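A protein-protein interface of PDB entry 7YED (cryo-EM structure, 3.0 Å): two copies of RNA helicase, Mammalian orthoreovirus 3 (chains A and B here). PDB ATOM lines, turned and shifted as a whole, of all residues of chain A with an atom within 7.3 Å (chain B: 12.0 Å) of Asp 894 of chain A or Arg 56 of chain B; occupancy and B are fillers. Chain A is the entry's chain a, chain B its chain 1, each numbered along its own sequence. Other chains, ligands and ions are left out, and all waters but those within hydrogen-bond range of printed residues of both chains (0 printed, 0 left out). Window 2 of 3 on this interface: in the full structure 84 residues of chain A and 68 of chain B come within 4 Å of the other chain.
The side-chain carboxylate of Asp 903 of chain A lies close to the side-chain hydroxyl of Tyr 53 of chain B.
The side-chain carboxylate (OD1) of Asp 894 of chain A lies within salt-bridge range of the guanidinium group (NH2) of Arg 56 of chain B (3.6 Å).
The backbone NH of Arg 56 of chain B sits close to the side-chain carboxylate of Asp 903 of chain A (3.3 Å).
The backbone carbonyl oxygen (O) of Tyr 53 of chain B lies close to the side-chain carboxylate (OE2) of Glu 51 of chain B (2.7 Å).
Among the printed residues, pairs that only touch across the chains: Asp 903 of chain A with Pro 57 of chain B, Val 899 of chain A with Tyr 53 of chain B, Trp 900 of chain A with Arg 56 of chain B, Gln 228 of chain A with Ile 59 of chain B, Ala 904 of chain A with Pro 57 of chain B, Val 899 of chain A with Arg 56 of chain B, Trp 900 of chain A with Pro 57 of chain B, Gln 228 of chain A with Tyr 53 of chain B and Ala 904 of chain A with Val 62 of chain B.
Of chain B, only Arg 56 (2.8 Å) comes within 4 Å of Asp 894 of chain A.
Arg 56 of chain B touches four residues of chain A.
No residue of chain B comes within 4 Å of Pro 892 of chain A.
Trp 900 of chain A touches two residues of chain B.
Asp 903 of chain A touches just these residues of chain B: Tyr 53 (2.4 Å), Arg 56 (3.2 Å) and Pro 57 (3.3 Å).
Of the printed residues of chain A, Pro 57 of chain B touches Trp 900, Asp 903 and Ala 904.
Of the printed residues of chain A, Ile 59 of chain B touches Gln 228.
Printed residues of chain A within 4 Å of Tyr 53 of chain B: Gln 228, Val 899 and Asp 903.
Of the printed residues of chain B, Ala 904 of chain A touches Pro 57 and Val 62.
Of the printed residues of chain B, Gln 228 of chain A touches Tyr 53 (3.8 Å) and Ile 59 (3.7 Å).
Tyr 891 of chain A touches none of the printed residues of chain B.
The nearest residue of chain A that does not touch Arg 56 of chain B is Leu 895 of chain A (4.6 Å).
The nearest printed residue of chain A that does not touch Pro 57 of chain B is Val 899 of chain A (5.4 Å).
Of the 13 printed residues of chain A, 6 touch a printed residue of chain B.
Printed residues of chain A that touch a printed residue of chain B: Gln 228, Asp 894, Val 899, Trp 900, Asp 903 and Ala 904.
Hydrophobic or aromatic side chains of chain A within 4 Å of the printed part of chain B: Val 899, Trp 900 and Ala 904.
Along chain A the printed residues that touch a printed residue of chain B span positions 228 to 904.
Hydrophobic or aromatic side chains of chain B within 4 Å of the printed part of chain A: Tyr 53, Pro 57, Ile 59 and Val 62.
Among the printed residues, Asp or Glu carboxylates within 4 Å of a Lys or Arg side-chain nitrogen of the other chain: Asp 894 of chain A with Arg 56 of chain B (3.6 Å).
No position is printed for both chains.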
ATOM      1  N   GLN A 228     -20.983   4.048 -23.445  1.00  0.00           N
ATOM      2  CA  GLN A 228     -21.919   4.329 -24.522  1.00  0.00           C
ATOM      3  C   GLN A 228     -21.133   4.877 -25.703  1.00  0.00           C
ATOM      4  O   GLN A 228     -19.902   4.964 -25.664  1.00  0.00           O
ATOM      5  CB  GLN A 228     -23.004   5.305 -24.061  1.00  0.00           C
ATOM      6  CG  GLN A 228     -22.476   6.676 -23.712  1.00  0.00           C
ATOM      7  CD  GLN A 228     -23.553   7.590 -23.187  1.00  0.00           C
ATOM      8  OE1 GLN A 228     -24.722   7.221 -23.137  1.00  0.00           O
ATOM      9  NE2 GLN A 228     -23.164   8.791 -22.786  1.00  0.00           N
ATOM     10  N   TYR A 891     -37.774   9.694  -5.039  1.00  0.00           N
ATOM     11  CA  TYR A 891     -36.774   9.197  -5.964  1.00  0.00           C
ATOM     12  C   TYR A 891     -37.446   8.285  -6.978  1.00  0.00           C
ATOM     13  O   TYR A 891     -38.541   7.770  -6.728  1.00  0.00           O
ATOM     14  CB  TYR A 891     -35.680   8.400  -5.243  1.00  0.00           C
ATOM     15  CG  TYR A 891     -34.766   9.195  -4.348  1.00  0.00           C
ATOM     16  CD1 TYR A 891     -34.763  10.575  -4.363  1.00  0.00           C
ATOM     17  CD2 TYR A 891     -33.877   8.549  -3.505  1.00  0.00           C
ATOM     18  CE1 TYR A 891     -33.915  11.289  -3.548  1.00  0.00           C
ATOM     19  CE2 TYR A 891     -33.032   9.252  -2.691  1.00  0.00           C
ATOM     20  CZ  TYR A 891     -33.052  10.620  -2.715  1.00  0.00           C
ATOM     21  OH  TYR A 891     -32.201  11.319  -1.899  1.00  0.00           O
ATOM     22  N   PRO A 892     -36.830   8.059  -8.135  1.00  0.00           N
ATOM     23  CA  PRO A 892     -37.306   6.992  -9.002  1.00  0.00           C
ATOM     24  C   PRO A 892     -37.165   5.654  -8.308  1.00  0.00           C
ATOM     25  O   PRO A 892     -36.221   5.438  -7.527  1.00  0.00           O
ATOM     26  CB  PRO A 892     -36.382   7.094 -10.225  1.00  0.00           C
ATOM     27  CG  PRO A 892     -35.906   8.488 -10.212  1.00  0.00           C
ATOM     28  CD  PRO A 892     -35.764   8.846  -8.771  1.00  0.00           C
ATOM     29  N   PRO A 893     -38.093   4.726  -8.547  1.00  0.00           N
ATOM     30  CA  PRO A 893     -38.055   3.446  -7.824  1.00  0.00           C
ATOM     31  C   PRO A 893     -36.795   2.634  -8.055  1.00  0.00           C
ATOM     32  O   PRO A 893     -36.455   1.802  -7.208  1.00  0.00           O
ATOM     33  CB  PRO A 893     -39.294   2.714  -8.349  1.00  0.00           C
ATOM     34  CG  PRO A 893     -40.201   3.795  -8.786  1.00  0.00           C
ATOM     35  CD  PRO A 893     -39.321   4.867  -9.343  1.00  0.00           C
ATOM     36  N   ASP A 894     -36.092   2.839  -9.163  1.00  0.00           N
ATOM     37  CA  ASP A 894     -34.832   2.148  -9.427  1.00  0.00           C
ATOM     38  C   ASP A 894     -33.737   3.194  -9.603  1.00  0.00           C
ATOM     39  O   ASP A 894     -33.383   3.572 -10.718  1.00  0.00           O
ATOM     40  CB  ASP A 894     -34.959   1.218 -10.653  1.00  0.00           C
ATOM     41  CG  ASP A 894     -35.435   1.934 -11.897  1.00  0.00           C
ATOM     42  OD1 ASP A 894     -35.758   3.136 -11.812  1.00  0.00           O
ATOM     43  OD2 ASP A 894     -35.471   1.292 -12.966  1.00  0.00           O
ATOM     44  N   LEU A 895     -33.180   3.647  -8.486  1.00  0.00           N
ATOM     45  CA  LEU A 895     -32.136   4.661  -8.500  1.00  0.00           C
ATOM     46  C   LEU A 895     -30.832   4.022  -8.055  1.00  0.00           C
ATOM     47  O   LEU A 895     -30.712   3.579  -6.908  1.00  0.00           O
ATOM     48  CB  LEU A 895     -32.493   5.845  -7.602  1.00  0.00           C
ATOM     49  CG  LEU A 895     -31.582   7.073  -7.692  1.00  0.00           C
ATOM     50  CD1 LEU A 895     -32.363   8.324  -7.379  1.00  0.00           C
ATOM     51  CD2 LEU A 895     -30.391   6.969  -6.760  1.00  0.00           C
ATOM     52  N   VAL A 896     -29.870   3.958  -8.965  1.00  0.00           N
ATOM     53  CA  VAL A 896     -28.498   3.593  -8.649  1.00  0.00           C
ATOM     54  C   VAL A 896     -27.672   4.854  -8.844  1.00  0.00           C
ATOM     55  O   VAL A 896     -27.517   5.333  -9.974  1.00  0.00           O
ATOM     56  CB  VAL A 896     -27.994   2.445  -9.529  1.00  0.00           C
ATOM     57  CG1 VAL A 896     -26.544   2.139  -9.215  1.00  0.00           C
ATOM     58  CG2 VAL A 896     -28.860   1.218  -9.333  1.00  0.00           C
ATOM     59  N   THR A 897     -27.158   5.403  -7.741  1.00  0.00           N
ATOM     60  CA  THR A 897     -26.545   6.724  -7.796  1.00  0.00           C
ATOM     61  C   THR A 897     -25.328   6.751  -8.706  1.00  0.00           C
ATOM     62  O   THR A 897     -25.083   7.761  -9.370  1.00  0.00           O
ATOM     63  CB  THR A 897     -26.151   7.182  -6.398  1.00  0.00           C
ATOM     64  OG1 THR A 897     -25.207   6.257  -5.850  1.00  0.00           O
ATOM     65  CG2 THR A 897     -27.367   7.243  -5.505  1.00  0.00           C
ATOM     66  N   VAL A 899     -24.816   5.081 -11.552  1.00  0.00           N
ATOM     67  CA  VAL A 899     -25.284   5.229 -12.926  1.00  0.00           C
ATOM     68  C   VAL A 899     -25.881   6.612 -13.144  1.00  0.00           C
ATOM     69  O   VAL A 899     -25.603   7.271 -14.152  1.00  0.00           O
ATOM     70  CB  VAL A 899     -26.297   4.122 -13.262  1.00  0.00           C
ATOM     71  CG1 VAL A 899     -26.854   4.327 -14.652  1.00  0.00           C
ATOM     72  CG2 VAL A 899     -25.648   2.764 -13.140  1.00  0.00           C
ATOM     73  N   TRP A 900     -26.708   7.073 -12.200  1.00  0.00           N
ATOM     74  CA  TRP A 900     -27.400   8.346 -12.378  1.00  0.00           C
ATOM     75  C   TRP A 900     -26.413   9.497 -12.507  1.00  0.00           C
ATOM     76  O   TRP A 900     -26.520  10.326 -13.417  1.00  0.00           O
ATOM     77  CB  TRP A 900     -28.352   8.599 -11.215  1.00  0.00           C
ATOM     78  CG  TRP A 900     -29.132   9.866 -11.357  1.00  0.00           C
ATOM     79  CD1 TRP A 900     -28.859  11.060 -10.774  1.00  0.00           C
ATOM     80  CD2 TRP A 900     -30.328  10.057 -12.119  1.00  0.00           C
ATOM     81  NE1 TRP A 900     -29.801  11.989 -11.130  1.00  0.00           N
ATOM     82  CE2 TRP A 900     -30.716  11.396 -11.956  1.00  0.00           C
ATOM     83  CE3 TRP A 900     -31.105   9.226 -12.927  1.00  0.00           C
ATOM     84  CZ2 TRP A 900     -31.843  11.924 -12.570  1.00  0.00           C
ATOM     85  CZ3 TRP A 900     -32.224   9.751 -13.535  1.00  0.00           C
ATOM     86  CH2 TRP A 900     -32.584  11.088 -13.353  1.00  0.00           C
ATOM     87  N   TYR A 901     -25.426   9.556 -11.620  1.00  0.00           N
ATOM     88  CA  TYR A 901     -24.510  10.682 -11.670  1.00  0.00           C
ATOM     89  C   TYR A 901     -23.447  10.509 -12.740  1.00  0.00           C
ATOM     90  O   TYR A 901     -22.956  11.507 -13.266  1.00  0.00           O
ATOM     91  CB  TYR A 901     -23.888  10.918 -10.298  1.00  0.00           C
ATOM     92  CG  TYR A 901     -24.907  11.416  -9.308  1.00  0.00           C
ATOM     93  CD1 TYR A 901     -25.313  12.738  -9.311  1.00  0.00           C
ATOM     94  CD2 TYR A 901     -25.483  10.561  -8.386  1.00  0.00           C
ATOM     95  CE1 TYR A 901     -26.252  13.195  -8.421  1.00  0.00           C
ATOM     96  CE2 TYR A 901     -26.422  11.010  -7.491  1.00  0.00           C
ATOM     97  CZ  TYR A 901     -26.803  12.329  -7.513  1.00  0.00           C
ATOM     98  OH  TYR A 901     -27.742  12.786  -6.622  1.00  0.00           O
ATOM     99  N   ASP A 903     -24.244   9.420 -15.644  1.00  0.00           N
ATOM    100  CA  ASP A 903     -24.956   9.920 -16.814  1.00  0.00           C
ATOM    101  C   ASP A 903     -25.199  11.420 -16.738  1.00  0.00           C
ATOM    102  O   ASP A 903     -25.277  12.082 -17.777  1.00  0.00           O
ATOM    103  CB  ASP A 903     -26.287   9.191 -16.977  1.00  0.00           C
ATOM    104  CG  ASP A 903     -26.112   7.750 -17.397  1.00  0.00           C
ATOM    105  OD1 ASP A 903     -25.106   7.441 -18.064  1.00  0.00           O
ATOM    106  OD2 ASP A 903     -26.987   6.924 -17.067  1.00  0.00           O
ATOM    107  N   ALA A 904     -25.331  11.971 -15.531  1.00  0.00           N
ATOM    108  CA  ALA A 904     -25.609  13.396 -15.407  1.00  0.00           C
ATOM    109  C   ALA A 904     -24.349  14.249 -15.495  1.00  0.00           C
ATOM    110  O   ALA A 904     -24.410  15.380 -15.983  1.00  0.00           O
ATOM    111  CB  ALA A 904     -26.339  13.674 -14.096  1.00  0.00           C
ATOM    112  N   GLU B  51     -26.985   1.140 -30.214  1.00  0.00           N
ATOM    113  CA  GLU B  51     -27.291   2.045 -29.100  1.00  0.00           C
ATOM    114  C   GLU B  51     -27.336   1.293 -27.774  1.00  0.00           C
ATOM    115  O   GLU B  51     -26.501   1.518 -26.894  1.00  0.00           O
ATOM    116  CB  GLU B  51     -28.614   2.760 -29.380  1.00  0.00           C
ATOM    117  CG  GLU B  51     -29.018   3.782 -28.334  1.00  0.00           C
ATOM    118  CD  GLU B  51     -28.074   4.967 -28.284  1.00  0.00           C
ATOM    119  OE1 GLU B  51     -27.427   5.253 -29.313  1.00  0.00           O
ATOM    120  OE2 GLU B  51     -27.979   5.614 -27.218  1.00  0.00           O
ATOM    121  N   HIS B  52     -28.312   0.399 -27.616  1.00  0.00           N
ATOM    122  CA  HIS B  52     -28.420  -0.484 -26.455  1.00  0.00           C
ATOM    123  C   HIS B  52     -28.576   0.223 -25.108  1.00  0.00           C
ATOM    124  O   HIS B  52     -28.649  -0.448 -24.073  1.00  0.00           O
ATOM    125  CB  HIS B  52     -27.200  -1.404 -26.371  1.00  0.00           C
ATOM    126  CG  HIS B  52     -27.088  -2.370 -27.506  1.00  0.00           C
ATOM    127  ND1 HIS B  52     -27.958  -3.426 -27.675  1.00  0.00           N
ATOM    128  CD2 HIS B  52     -26.180  -2.469 -28.505  1.00  0.00           C
ATOM    129  CE1 HIS B  52     -27.606  -4.117 -28.744  1.00  0.00           C
ATOM    130  NE2 HIS B  52     -26.529  -3.557 -29.266  1.00  0.00           N
ATOM    131  N   TYR B  53     -28.634   1.553 -25.085  1.00  0.00           N
ATOM    132  CA  TYR B  53     -28.622   2.265 -23.810  1.00  0.00           C
ATOM    133  C   TYR B  53     -29.076   3.698 -24.020  1.00  0.00           C
ATOM    134  O   TYR B  53     -28.450   4.441 -24.780  1.00  0.00           O
ATOM    135  CB  TYR B  53     -27.229   2.236 -23.188  1.00  0.00           C
ATOM    136  CG  TYR B  53     -27.158   2.935 -21.854  1.00  0.00           C
ATOM    137  CD1 TYR B  53     -27.708   2.358 -20.721  1.00  0.00           C
ATOM    138  CD2 TYR B  53     -26.552   4.171 -21.727  1.00  0.00           C
ATOM    139  CE1 TYR B  53     -27.651   2.992 -19.504  1.00  0.00           C
ATOM    140  CE2 TYR B  53     -26.491   4.812 -20.514  1.00  0.00           C
ATOM    141  CZ  TYR B  53     -27.043   4.218 -19.405  1.00  0.00           C
ATOM    142  OH  TYR B  53     -26.984   4.856 -18.189  1.00  0.00           O
ATOM    143  N   LYS B  54     -30.144   4.085 -23.335  1.00  0.00           N
ATOM    144  CA  LYS B  54     -30.579   5.471 -23.269  1.00  0.00           C
ATOM    145  C   LYS B  54     -30.194   6.031 -21.906  1.00  0.00           C
ATOM    146  O   LYS B  54     -30.470   5.405 -20.878  1.00  0.00           O
ATOM    147  CB  LYS B  54     -32.087   5.584 -23.495  1.00  0.00           C
ATOM    148  CG  LYS B  54     -32.929   4.924 -22.419  1.00  0.00           C
ATOM    149  CD  LYS B  54     -34.412   5.034 -22.733  1.00  0.00           C
ATOM    150  CE  LYS B  54     -35.261   4.446 -21.615  1.00  0.00           C
ATOM    151  NZ  LYS B  54     -35.086   2.977 -21.465  1.00  0.00           N
ATOM    152  N   ALA B  55     -29.542   7.189 -21.904  1.00  0.00           N
ATOM    153  CA  ALA B  55     -29.029   7.759 -20.666  1.00  0.00           C
ATOM    154  C   ALA B  55     -30.165   8.036 -19.687  1.00  0.00           C
ATOM    155  O   ALA B  55     -31.316   8.249 -20.073  1.00  0.00           O
ATOM    156  CB  ALA B  55     -28.250   9.041 -20.953  1.00  0.00           C
ATOM    157  N   ARG B  56     -29.829   8.025 -18.398  1.00  0.00           N
ATOM    158  CA  ARG B  56     -30.856   8.097 -17.367  1.00  0.00           C
ATOM    159  C   ARG B  56     -31.418   9.508 -17.250  1.00  0.00           C
ATOM    160  O   ARG B  56     -32.636   9.685 -17.380  1.00  0.00           O
ATOM    161  CB  ARG B  56     -30.313   7.601 -16.024  1.00  0.00           C
ATOM    162  CG  ARG B  56     -29.900   6.134 -16.008  1.00  0.00           C
ATOM    163  CD  ARG B  56     -31.103   5.215 -16.155  1.00  0.00           C
ATOM    164  NE  ARG B  56     -32.084   5.413 -15.091  1.00  0.00           N
ATOM    165  CZ  ARG B  56     -32.045   4.809 -13.909  1.00  0.00           C
ATOM    166  NH1 ARG B  56     -31.066   3.957 -13.628  1.00  0.00           N
ATOM    167  NH2 ARG B  56     -32.985   5.056 -13.007  1.00  0.00           N
ATOM    168  N   PRO B  57     -30.601  10.539 -16.997  1.00  0.00           N
ATOM    169  CA  PRO B  57     -31.161  11.900 -17.019  1.00  0.00           C
ATOM    170  C   PRO B  57     -31.525  12.371 -18.414  1.00  0.00           C
ATOM    171  O   PRO B  57     -32.603  12.945 -18.603  1.00  0.00           O
ATOM    172  CB  PRO B  57     -30.042  12.753 -16.405  1.00  0.00           C
ATOM    173  CG  PRO B  57     -29.228  11.806 -15.629  1.00  0.00           C
ATOM    174  CD  PRO B  57     -29.249  10.537 -16.419  1.00  0.00           C
ATOM    175  N   GLY B  58     -30.663  12.142 -19.398  1.00  0.00           N
ATOM    176  CA  GLY B  58     -30.930  12.604 -20.743  1.00  0.00           C
ATOM    177  C   GLY B  58     -29.896  13.591 -21.244  1.00  0.00           C
ATOM    178  O   GLY B  58     -29.823  14.731 -20.764  1.00  0.00           O
ATOM    179  N   ILE B  59     -29.095  13.156 -22.219  1.00  0.00           N
ATOM    180  CA  ILE B  59     -27.989  13.973 -22.704  1.00  0.00           C
ATOM    181  C   ILE B  59     -28.501  15.279 -23.291  1.00  0.00           C
ATOM    182  O   ILE B  59     -27.916  16.342 -23.069  1.00  0.00           O
ATOM    183  CB  ILE B  59     -27.150  13.192 -23.729  1.00  0.00           C
ATOM    184  CG1 ILE B  59     -26.520  11.965 -23.081  1.00  0.00           C
ATOM    185  CG2 ILE B  59     -26.073  14.082 -24.311  1.00  0.00           C
ATOM    186  CD1 ILE B  59     -25.862  11.039 -24.068  1.00  0.00           C
ATOM    187  N   ALA B  60     -29.601  15.224 -24.039  1.00  0.00           N
ATOM    188  CA  ALA B  60     -30.104  16.425 -24.698  1.00  0.00           C
ATOM    189  C   ALA B  60     -30.560  17.464 -23.681  1.00  0.00           C
ATOM    190  O   ALA B  60     -30.208  18.645 -23.786  1.00  0.00           O
ATOM    191  CB  ALA B  60     -31.243  16.061 -25.648  1.00  0.00           C
ATOM    192  N   SER B  61     -31.344  17.044 -22.689  1.00  0.00           N
ATOM    193  CA  SER B  61     -31.836  17.994 -21.699  1.00  0.00           C
ATOM    194  C   SER B  61     -30.699  18.544 -20.849  1.00  0.00           C
ATOM    195  O   SER B  61     -30.667  19.744 -20.549  1.00  0.00           O
ATOM    196  CB  SER B  61     -32.895  17.337 -20.820  1.00  0.00           C
ATOM    197  OG  SER B  61     -32.328  16.312 -20.028  1.00  0.00           O
ATOM    198  N   VAL B  62     -29.756  17.684 -20.454  1.00  0.00           N
ATOM    199  CA  VAL B  62     -28.628  18.158 -19.658  1.00  0.00           C
ATOM    200  C   VAL B  62     -27.792  19.151 -20.456  1.00  0.00           C
ATOM    201  O   VAL B  62     -27.332  20.166 -19.920  1.00  0.00           O
ATOM    202  CB  VAL B  62     -27.780  16.973 -19.168  1.00  0.00           C
ATOM    203  CG1 VAL B  62     -26.571  17.480 -18.415  1.00  0.00           C
ATOM    204  CG2 VAL B  62     -28.608  16.063 -18.289  1.00  0.00           C
ATOM    205  N   GLN B  63     -27.592  18.885 -21.750  1.00  0.00           N
ATOM    206  CA  GLN B  63     -26.836  19.812 -22.583  1.00  0.00           C
ATOM    207  C   GLN B  63     -27.561  21.138 -22.733  1.00  0.00           C
ATOM    208  O   GLN B  63     -26.930  22.197 -22.703  1.00  0.00           O
ATOM    209  CB  GLN B  63     -26.569  19.206 -23.957  1.00  0.00           C
ATOM    210  CG  GLN B  63     -25.580  18.065 -23.964  1.00  0.00           C
ATOM    211  CD  GLN B  63     -25.362  17.505 -25.351  1.00  0.00           C
ATOM    212  OE1 GLN B  63     -26.015  17.920 -26.307  1.00  0.00           O
ATOM    213  NE2 GLN B  63     -24.440  16.563 -25.472  1.00  0.00           N
